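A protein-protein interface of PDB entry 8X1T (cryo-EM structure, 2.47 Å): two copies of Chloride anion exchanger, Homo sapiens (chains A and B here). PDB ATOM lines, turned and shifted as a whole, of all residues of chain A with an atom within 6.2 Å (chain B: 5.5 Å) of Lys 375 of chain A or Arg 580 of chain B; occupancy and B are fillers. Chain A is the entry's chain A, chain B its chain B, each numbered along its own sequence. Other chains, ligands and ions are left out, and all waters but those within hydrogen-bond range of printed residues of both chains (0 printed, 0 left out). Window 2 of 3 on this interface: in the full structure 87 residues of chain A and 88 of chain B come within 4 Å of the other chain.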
ATOM      1  N   SER A 370      -5.569  26.436   8.640  1.00  0.00           N
ATOM      2  CA  SER A 370      -4.894  26.640   9.913  1.00  0.00           C
ATOM      3  C   SER A 370      -5.753  27.304  10.961  1.00  0.00           C
ATOM      4  O   SER A 370      -5.448  27.252  12.138  1.00  0.00           O
ATOM      5  CB  SER A 370      -3.640  27.468   9.708  1.00  0.00           C
ATOM      6  OG  SER A 370      -2.799  26.846   8.770  1.00  0.00           O
ATOM      7  N   VAL A 371      -6.826  27.939  10.532  1.00  0.00           N
ATOM      8  CA  VAL A 371      -7.720  28.602  11.451  1.00  0.00           C
ATOM      9  C   VAL A 371      -8.634  27.583  12.089  1.00  0.00           C
ATOM     10  O   VAL A 371      -9.114  27.795  13.185  1.00  0.00           O
ATOM     11  CB  VAL A 371      -8.584  29.643  10.731  1.00  0.00           C
ATOM     12  CG1 VAL A 371      -9.768  30.034  11.587  1.00  0.00           C
ATOM     13  CG2 VAL A 371      -7.753  30.854  10.362  1.00  0.00           C
ATOM     14  N   TYR A 372      -8.864  26.473  11.397  1.00  0.00           N
ATOM     15  CA  TYR A 372      -9.745  25.417  11.872  1.00  0.00           C
ATOM     16  C   TYR A 372      -9.001  24.264  12.500  1.00  0.00           C
ATOM     17  O   TYR A 372      -9.589  23.484  13.220  1.00  0.00           O
ATOM     18  CB  TYR A 372     -10.636  24.916  10.744  1.00  0.00           C
ATOM     19  CG  TYR A 372     -11.542  25.975  10.194  1.00  0.00           C
ATOM     20  CD1 TYR A 372     -12.489  26.581  10.995  1.00  0.00           C
ATOM     21  CD2 TYR A 372     -11.453  26.371   8.876  1.00  0.00           C
ATOM     22  CE1 TYR A 372     -13.317  27.558  10.500  1.00  0.00           C
ATOM     23  CE2 TYR A 372     -12.285  27.344   8.371  1.00  0.00           C
ATOM     24  CZ  TYR A 372     -13.211  27.930   9.191  1.00  0.00           C
ATOM     25  OH  TYR A 372     -14.037  28.903   8.703  1.00  0.00           O
ATOM     26  N   SER A 373      -7.717  24.129  12.199  1.00  0.00           N
ATOM     27  CA  SER A 373      -6.899  23.089  12.804  1.00  0.00           C
ATOM     28  C   SER A 373      -6.744  23.517  14.228  1.00  0.00           C
ATOM     29  O   SER A 373      -6.906  22.736  15.157  1.00  0.00           O
ATOM     30  CB  SER A 373      -5.519  23.049  12.180  1.00  0.00           C
ATOM     31  OG  SER A 373      -5.608  22.980  10.781  1.00  0.00           O
ATOM     32  N   LEU A 374      -6.406  24.784  14.383  1.00  0.00           N
ATOM     33  CA  LEU A 374      -6.236  25.396  15.666  1.00  0.00           C
ATOM     34  C   LEU A 374      -7.569  25.428  16.379  1.00  0.00           C
ATOM     35  O   LEU A 374      -7.649  25.051  17.531  1.00  0.00           O
ATOM     36  CB  LEU A 374      -5.708  26.807  15.482  1.00  0.00           C
ATOM     37  CG  LEU A 374      -5.304  27.552  16.740  1.00  0.00           C
ATOM     38  CD1 LEU A 374      -4.109  26.882  17.385  1.00  0.00           C
ATOM     39  CD2 LEU A 374      -4.979  28.987  16.380  1.00  0.00           C
ATOM     40  N   LYS A 375      -8.634  25.851  15.706  1.00  0.00           N
ATOM     41  CA  LYS A 375      -9.915  25.915  16.399  1.00  0.00           C
ATOM     42  C   LYS A 375     -10.367  24.543  16.883  1.00  0.00           C
ATOM     43  O   LYS A 375     -11.008  24.436  17.934  1.00  0.00           O
ATOM     44  CB  LYS A 375     -10.971  26.533  15.486  1.00  0.00           C
ATOM     45  CG  LYS A 375     -12.328  26.722  16.131  1.00  0.00           C
ATOM     46  CD  LYS A 375     -13.276  27.428  15.188  1.00  0.00           C
ATOM     47  CE  LYS A 375     -14.431  28.057  15.936  1.00  0.00           C
ATOM     48  NZ  LYS A 375     -15.407  27.048  16.410  1.00  0.00           N
ATOM     49  N   TYR A 376     -10.054  23.482  16.140  1.00  0.00           N
ATOM     50  CA  TYR A 376     -10.537  22.149  16.480  1.00  0.00           C
ATOM     51  C   TYR A 376      -9.426  21.178  16.854  1.00  0.00           C
ATOM     52  O   TYR A 376      -9.705  19.998  17.090  1.00  0.00           O
ATOM     53  CB  TYR A 376     -11.371  21.585  15.331  1.00  0.00           C
ATOM     54  CG  TYR A 376     -12.591  22.420  15.040  1.00  0.00           C
ATOM     55  CD1 TYR A 376     -12.557  23.413  14.080  1.00  0.00           C
ATOM     56  CD2 TYR A 376     -13.766  22.236  15.746  1.00  0.00           C
ATOM     57  CE1 TYR A 376     -13.654  24.184  13.822  1.00  0.00           C
ATOM     58  CE2 TYR A 376     -14.871  23.003  15.492  1.00  0.00           C
ATOM     59  CZ  TYR A 376     -14.809  23.976  14.527  1.00  0.00           C
ATOM     60  OH  TYR A 376     -15.908  24.753  14.262  1.00  0.00           O
ATOM     61  N   ASP A 377      -8.178  21.641  16.915  1.00  0.00           N
ATOM     62  CA  ASP A 377      -7.073  20.891  17.516  1.00  0.00           C
ATOM     63  C   ASP A 377      -6.835  19.556  16.810  1.00  0.00           C
ATOM     64  O   ASP A 377      -7.056  18.478  17.363  1.00  0.00           O
ATOM     65  CB  ASP A 377      -7.321  20.687  19.014  1.00  0.00           C
ATOM     66  CG  ASP A 377      -6.060  20.319  19.773  1.00  0.00           C
ATOM     67  OD1 ASP A 377      -5.377  19.353  19.382  1.00  0.00           O
ATOM     68  OD2 ASP A 377      -5.749  21.009  20.766  1.00  0.00           O
ATOM     69  N   GLU A 415     -18.351  25.007   7.777  1.00  0.00           N
ATOM     70  CA  GLU A 415     -18.045  24.844   9.191  1.00  0.00           C
ATOM     71  C   GLU A 415     -19.166  25.350  10.090  1.00  0.00           C
ATOM     72  O   GLU A 415     -19.501  24.711  11.082  1.00  0.00           O
ATOM     73  CB  GLU A 415     -16.714  25.527   9.522  1.00  0.00           C
ATOM     74  CG  GLU A 415     -16.313  25.461  10.984  1.00  0.00           C
ATOM     75  CD  GLU A 415     -16.910  26.590  11.795  1.00  0.00           C
ATOM     76  OE1 GLU A 415     -17.254  27.632  11.200  1.00  0.00           O
ATOM     77  OE2 GLU A 415     -17.034  26.443  13.024  1.00  0.00           O
ATOM     78  N   PRO B 575      -0.239  24.387  26.096  1.00  0.00           N
ATOM     79  CA  PRO B 575      -1.048  25.073  27.116  1.00  0.00           C
ATOM     80  C   PRO B 575      -2.507  25.252  26.729  1.00  0.00           C
ATOM     81  O   PRO B 575      -3.373  25.183  27.610  1.00  0.00           O
ATOM     82  CB  PRO B 575      -0.341  26.424  27.272  1.00  0.00           C
ATOM     83  CG  PRO B 575       0.496  26.574  26.056  1.00  0.00           C
ATOM     84  CD  PRO B 575       0.906  25.201  25.667  1.00  0.00           C
ATOM     85  N   LEU B 576      -2.808  25.457  25.450  1.00  0.00           N
ATOM     86  CA  LEU B 576      -4.190  25.551  24.997  1.00  0.00           C
ATOM     87  C   LEU B 576      -4.937  24.231  25.146  1.00  0.00           C
ATOM     88  O   LEU B 576      -6.117  24.233  25.503  1.00  0.00           O
ATOM     89  CB  LEU B 576      -4.235  26.011  23.540  1.00  0.00           C
ATOM     90  CG  LEU B 576      -5.582  26.516  23.033  1.00  0.00           C
ATOM     91  CD1 LEU B 576      -6.153  27.557  23.971  1.00  0.00           C
ATOM     92  CD2 LEU B 576      -5.426  27.085  21.642  1.00  0.00           C
ATOM     93  N   ARG B 577      -4.271  23.104  24.897  1.00  0.00           N
ATOM     94  CA  ARG B 577      -4.910  21.804  25.075  1.00  0.00           C
ATOM     95  C   ARG B 577      -5.196  21.524  26.546  1.00  0.00           C
ATOM     96  O   ARG B 577      -6.260  20.994  26.892  1.00  0.00           O
ATOM     97  CB  ARG B 577      -4.029  20.711  24.484  1.00  0.00           C
ATOM     98  CG  ARG B 577      -4.673  19.347  24.411  1.00  0.00           C
ATOM     99  CD  ARG B 577      -3.922  18.470  23.435  1.00  0.00           C
ATOM    100  NE  ARG B 577      -3.265  19.278  22.414  1.00  0.00           N
ATOM    101  CZ  ARG B 577      -2.436  18.798  21.497  1.00  0.00           C
ATOM    102  NH1 ARG B 577      -2.155  17.505  21.468  1.00  0.00           N
ATOM    103  NH2 ARG B 577      -1.887  19.613  20.608  1.00  0.00           N
ATOM    104  N   ILE B 578      -4.256  21.870  27.427  1.00  0.00           N
ATOM    105  CA  ILE B 578      -4.486  21.708  28.859  1.00  0.00           C
ATOM    106  C   ILE B 578      -5.638  22.590  29.311  1.00  0.00           C
ATOM    107  O   ILE B 578      -6.483  22.174  30.108  1.00  0.00           O
ATOM    108  CB  ILE B 578      -3.204  22.013  29.654  1.00  0.00           C
ATOM    109  CG1 ILE B 578      -2.031  21.204  29.109  1.00  0.00           C
ATOM    110  CG2 ILE B 578      -3.412  21.709  31.120  1.00  0.00           C
ATOM    111  CD1 ILE B 578      -1.986  19.791  29.602  1.00  0.00           C
ATOM    112  N   LEU B 579      -5.697  23.821  28.801  1.00  0.00           N
ATOM    113  CA  LEU B 579      -6.793  24.714  29.164  1.00  0.00           C
ATOM    114  C   LEU B 579      -8.129  24.183  28.665  1.00  0.00           C
ATOM    115  O   LEU B 579      -9.134  24.255  29.380  1.00  0.00           O
ATOM    116  CB  LEU B 579      -6.533  26.110  28.612  1.00  0.00           C
ATOM    117  CG  LEU B 579      -7.680  27.104  28.743  1.00  0.00           C
ATOM    118  CD1 LEU B 579      -7.993  27.368  30.198  1.00  0.00           C
ATOM    119  CD2 LEU B 579      -7.332  28.381  28.018  1.00  0.00           C
ATOM    120  N   ARG B 580      -8.163  23.637  27.450  1.00  0.00           N
ATOM    121  CA  ARG B 580      -9.408  23.101  26.910  1.00  0.00           C
ATOM    122  C   ARG B 580      -9.881  21.888  27.696  1.00  0.00           C
ATOM    123  O   ARG B 580     -11.078  21.744  27.960  1.00  0.00           O
ATOM    124  CB  ARG B 580      -9.228  22.745  25.440  1.00  0.00           C
ATOM    125  CG  ARG B 580      -9.327  23.931  24.521  1.00  0.00           C
ATOM    126  CD  ARG B 580      -8.755  23.626  23.162  1.00  0.00           C
ATOM    127  NE  ARG B 580      -8.948  24.739  22.244  1.00  0.00           N
ATOM    128  CZ  ARG B 580      -8.299  24.874  21.094  1.00  0.00           C
ATOM    129  NH1 ARG B 580      -7.414  23.963  20.722  1.00  0.00           N
ATOM    130  NH2 ARG B 580      -8.533  25.920  20.319  1.00  0.00           N
ATOM    131  N   LYS B 581      -8.961  21.005  28.087  1.00  0.00           N
ATOM    132  CA  LYS B 581      -9.376  19.848  28.873  1.00  0.00           C
ATOM    133  C   LYS B 581      -9.783  20.244  30.286  1.00  0.00           C
ATOM    134  O   LYS B 581     -10.701  19.643  30.857  1.00  0.00           O
ATOM    135  CB  LYS B 581      -8.266  18.803  28.889  1.00  0.00           C
ATOM    136  CG  LYS B 581      -7.950  18.275  27.502  1.00  0.00           C
ATOM    137  CD  LYS B 581      -7.164  16.984  27.544  1.00  0.00           C
ATOM    138  CE  LYS B 581      -6.651  16.618  26.162  1.00  0.00           C
ATOM    139  NZ  LYS B 581      -5.812  15.393  26.185  1.00  0.00           N
ATOM    140  N   ARG B 582      -9.147  21.272  30.854  1.00  0.00           N
ATOM    141  CA  ARG B 582      -9.593  21.788  32.146  1.00  0.00           C
ATOM    142  C   ARG B 582     -10.983  22.397  32.042  1.00  0.00           C
ATOM    143  O   ARG B 582     -11.804  22.239  32.950  1.00  0.00           O
ATOM    144  CB  ARG B 582      -8.594  22.813  32.674  1.00  0.00           C
ATOM    145  CG  ARG B 582      -7.309  22.204  33.181  1.00  0.00           C
ATOM    146  CD  ARG B 582      -6.390  23.237  33.792  1.00  0.00           C
ATOM    147  NE  ARG B 582      -5.138  22.625  34.218  1.00  0.00           N
ATOM    148  CZ  ARG B 582      -4.159  23.273  34.837  1.00  0.00           C
ATOM    149  NH1 ARG B 582      -4.285  24.562  35.108  1.00  0.00           N
ATOM    150  NH2 ARG B 582      -3.057  22.631  35.190  1.00  0.00           N
ATOM    151  N   ASN B 583     -11.267  23.091  30.941  1.00  0.00           N
ATOM    152  CA  ASN B 583     -12.589  23.678  30.750  1.00  0.00           C
ATOM    153  C   ASN B 583     -13.648  22.602  30.542  1.00  0.00           C
ATOM    154  O   ASN B 583     -14.777  22.734  31.027  1.00  0.00           O
ATOM    155  CB  ASN B 583     -12.562  24.649  29.575  1.00  0.00           C
ATOM    156  CG  ASN B 583     -12.378  26.082  30.010  1.00  0.00           C
ATOM    157  OD1 ASN B 583     -12.978  26.523  30.984  1.00  0.00           O
ATOM    158  ND2 ASN B 583     -11.551  26.818  29.285  1.00  0.00           N
ATOM    159  N   LYS B 584     -13.303  21.527  29.831  1.00  0.00           N
ATOM    160  CA  LYS B 584     -14.212  20.389  29.716  1.00  0.00           C
ATOM    161  C   LYS B 584     -14.503  19.784  31.082  1.00  0.00           C
ATOM    162  O   LYS B 584     -15.657  19.490  31.416  1.00  0.00           O
ATOM    163  CB  LYS B 584     -13.618  19.333  28.790  1.00  0.00           C
ATOM    164  CG  LYS B 584     -13.940  19.520  27.331  1.00  0.00           C
ATOM    165  CD  LYS B 584     -13.524  18.298  26.531  1.00  0.00           C
ATOM    166  CE  LYS B 584     -12.025  18.277  26.289  1.00  0.00           C
ATOM    167  NZ  LYS B 584     -11.600  19.294  25.287  1.00  0.00           N
ATOM    168  N   ALA B 585     -13.454  19.569  31.883  1.00  0.00           N
ATOM    169  CA  ALA B 585     -13.641  19.009  33.215  1.00  0.00           C
ATOM    170  C   ALA B 585     -14.499  19.919  34.083  1.00  0.00           C
ATOM    171  O   ALA B 585     -15.333  19.443  34.856  1.00  0.00           O
ATOM    172  CB  ALA B 585     -12.287  18.763  33.874  1.00  0.00           C
ATOM    173  N   ASN B 621     -19.952  23.344  16.576  1.00  0.00           N
ATOM    174  CA  ASN B 621     -18.905  24.181  16.012  1.00  0.00           C
ATOM    175  C   ASN B 621     -19.000  25.623  16.479  1.00  0.00           C
ATOM    176  O   ASN B 621     -17.993  26.315  16.558  1.00  0.00           O
ATOM    177  CB  ASN B 621     -18.959  24.122  14.484  1.00  0.00           C
ATOM    178  CG  ASN B 621     -18.699  22.730  13.942  1.00  0.00           C
ATOM    179  OD1 ASN B 621     -18.669  21.755  14.690  1.00  0.00           O
ATOM    180  ND2 ASN B 621     -18.507  22.632  12.634  1.00  0.00           N
ATOM    181  N   ASN B 622     -20.205  26.080  16.786  1.00  0.00           N
ATOM    182  CA  ASN B 622     -20.401  27.463  17.206  1.00  0.00           C
ATOM    183  C   ASN B 622     -20.330  27.631  18.716  1.00  0.00           C
ATOM    184  O   ASN B 622     -20.462  28.740  19.222  1.00  0.00           O
ATOM    185  CB  ASN B 622     -21.743  27.972  16.683  1.00  0.00           C
ATOM    186  CG  ASN B 622     -21.804  28.009  15.168  1.00  0.00           C
ATOM    187  OD1 ASN B 622     -22.882  28.083  14.581  1.00  0.00           O
ATOM    188  ND2 ASN B 622     -20.643  27.952  14.524  1.00  0.00           N
ATOM    189  N   ILE B 624     -17.903  25.450  20.531  1.00  0.00           N
ATOM    190  CA  ILE B 624     -16.652  24.844  20.976  1.00  0.00           C
ATOM    191  C   ILE B 624     -15.611  25.854  21.458  1.00  0.00           C
ATOM    192  O   ILE B 624     -14.666  25.487  22.142  1.00  0.00           O
ATOM    193  CB  ILE B 624     -16.049  23.954  19.862  1.00  0.00           C
ATOM    194  CG1 ILE B 624     -15.037  22.970  20.454  1.00  0.00           C
ATOM    195  CG2 ILE B 624     -15.425  24.809  18.769  1.00  0.00           C
ATOM    196  CD1 ILE B 624     -14.415  22.049  19.431  1.00  0.00           C
ATOM    197  N   GLU B 625     -15.796  27.125  21.131  1.00  0.00           N
ATOM    198  CA  GLU B 625     -14.812  28.142  21.498  1.00  0.00           C
ATOM    199  C   GLU B 625     -14.909  28.571  22.957  1.00  0.00           C
ATOM    200  O   GLU B 625     -14.104  29.373  23.422  1.00  0.00           O
ATOM    201  CB  GLU B 625     -14.955  29.362  20.591  1.00  0.00           C
ATOM    202  CG  GLU B 625     -16.309  30.045  20.676  1.00  0.00           C
ATOM    203  CD  GLU B 625     -16.398  31.262  19.777  1.00  0.00           C
ATOM    204  OE1 GLU B 625     -15.380  31.611  19.144  1.00  0.00           O
ATOM    205  OE2 GLU B 625     -17.485  31.873  19.702  1.00  0.00           O
ATOM    206  N   LEU B 627     -14.256  26.742  25.255  1.00  0.00           N
ATOM    207  CA  LEU B 627     -13.207  26.005  25.949  1.00  0.00           C
ATOM    208  C   LEU B 627     -11.863  26.737  25.989  1.00  0.00           C
ATOM    209  O   LEU B 627     -10.949  26.282  26.664  1.00  0.00           O
ATOM    210  CB  LEU B 627     -13.041  24.609  25.345  1.00  0.00           C
ATOM    211  CG  LEU B 627     -14.271  23.703  25.406  1.00  0.00           C
ATOM    212  CD1 LEU B 627     -13.960  22.344  24.799  1.00  0.00           C
ATOM    213  CD2 LEU B 627     -14.765  23.550  26.835  1.00  0.00           C
ATOM    214  N   ASP B 628     -11.729  27.858  25.290  1.00  0.00           N
ATOM    215  CA  ASP B 628     -10.498  28.628  25.394  1.00  0.00           C
ATOM    216  C   ASP B 628     -10.616  29.809  26.346  1.00  0.00           C
ATOM    217  O   ASP B 628      -9.701  30.636  26.401  1.00  0.00           O
ATOM    218  CB  ASP B 628     -10.066  29.133  24.018  1.00  0.00           C
ATOM    219  CG  ASP B 628     -10.092  28.055  22.972  1.00  0.00           C
ATOM    220  OD1 ASP B 628     -10.334  28.378  21.793  1.00  0.00           O
ATOM    221  OD2 ASP B 628      -9.871  26.881  23.325  1.00  0.00           O
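The side-chain amino group (NZ) of Lys 375 of chain A is in hydrogen-bond range of the side-chain hydroxyl (OH) of Tyr 376 of chain A.
NZ of Lys 375 of chain A lies within salt-bridge range of OE2 of Glu 415 of chain A, 3.8 Å away.
NE of Arg 580 of chain B is in salt-bridge range of OD2 of Asp 628 of chain B, at 2.6 Å.
No position is printed for both chains.
Of the 9 pairs that touch across the chains among the printed residues, none has its exchanged pair printed and touching as well.
Ser 370 of chain A touches none of the printed residues of chain B.
Of the printed residues of chain B, Tyr 376 of chain A touches Asn 621 (3.1 Å) and Ile 624 (3.7 Å).
Printed residues of chain B within 4 Å of Glu 415 of chain A: Asn 621.
Of the printed residues of chain A, Asn 621 of chain B touches Lys 375 (2.7 Å), Tyr 376 (3.1 Å) and Glu 415 (2.8 Å).
Printed residues of chain A within 4 Å of Ile 624 of chain B: Lys 375 (3.3 Å) and Tyr 376 (3.7 Å).
Leu 627 of chain B touches none of the printed residues of chain A.
The nearest residue of chain B that does not touch Lys 375 of chain A is Glu 625 of chain B (4.7 Å).
Among the printed residues, pairs that only touch across the chains: Lys 375 of chain A with Ile 624 of chain B (3.3 Å), Lys 375 of chain A with Arg 580 of chain B (3.7 Å) and Tyr 376 of chain A with Ile 624 of chain B (3.7 Å).
The backbone carbonyl oxygen of Leu 374 of chain A sits at hydrogen-bond distance from the guanidinium group of Arg 580 of chain B (3.1 Å).
The side-chain amino group (NZ) of Lys 375 of chain A lies within hydrogen-bond range of the backbone carbonyl oxygen (O) of Asn 621 of chain B (2.7 Å).
O of Asn 621 of chain B lies close to OH of Tyr 376 of chain A (3.5 Å).
OD2 of Asp 377 of chain A is in salt-bridge range of NE of Arg 577 of chain B (3.4 Å).
OD2 of Asp 377 of chain A is in salt-bridge range of NH1 of Arg 580 of chain B, 3.4 Å away.
The backbone carbonyl oxygen (O) of Glu 415 of chain A is in hydrogen-bond range of the side-chain amide nitrogen (ND2) of Asn 621 of chain B (2.8 Å).
Hydrophobic or aromatic side chains of chain B within 4 Å of the printed part of chain A: Ile 624.
Hydrophobic or aromatic side chains of chain A within 4 Å of the printed part of chain B: Tyr 376.
Among the printed residues, 9 pairs touch across the chains.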
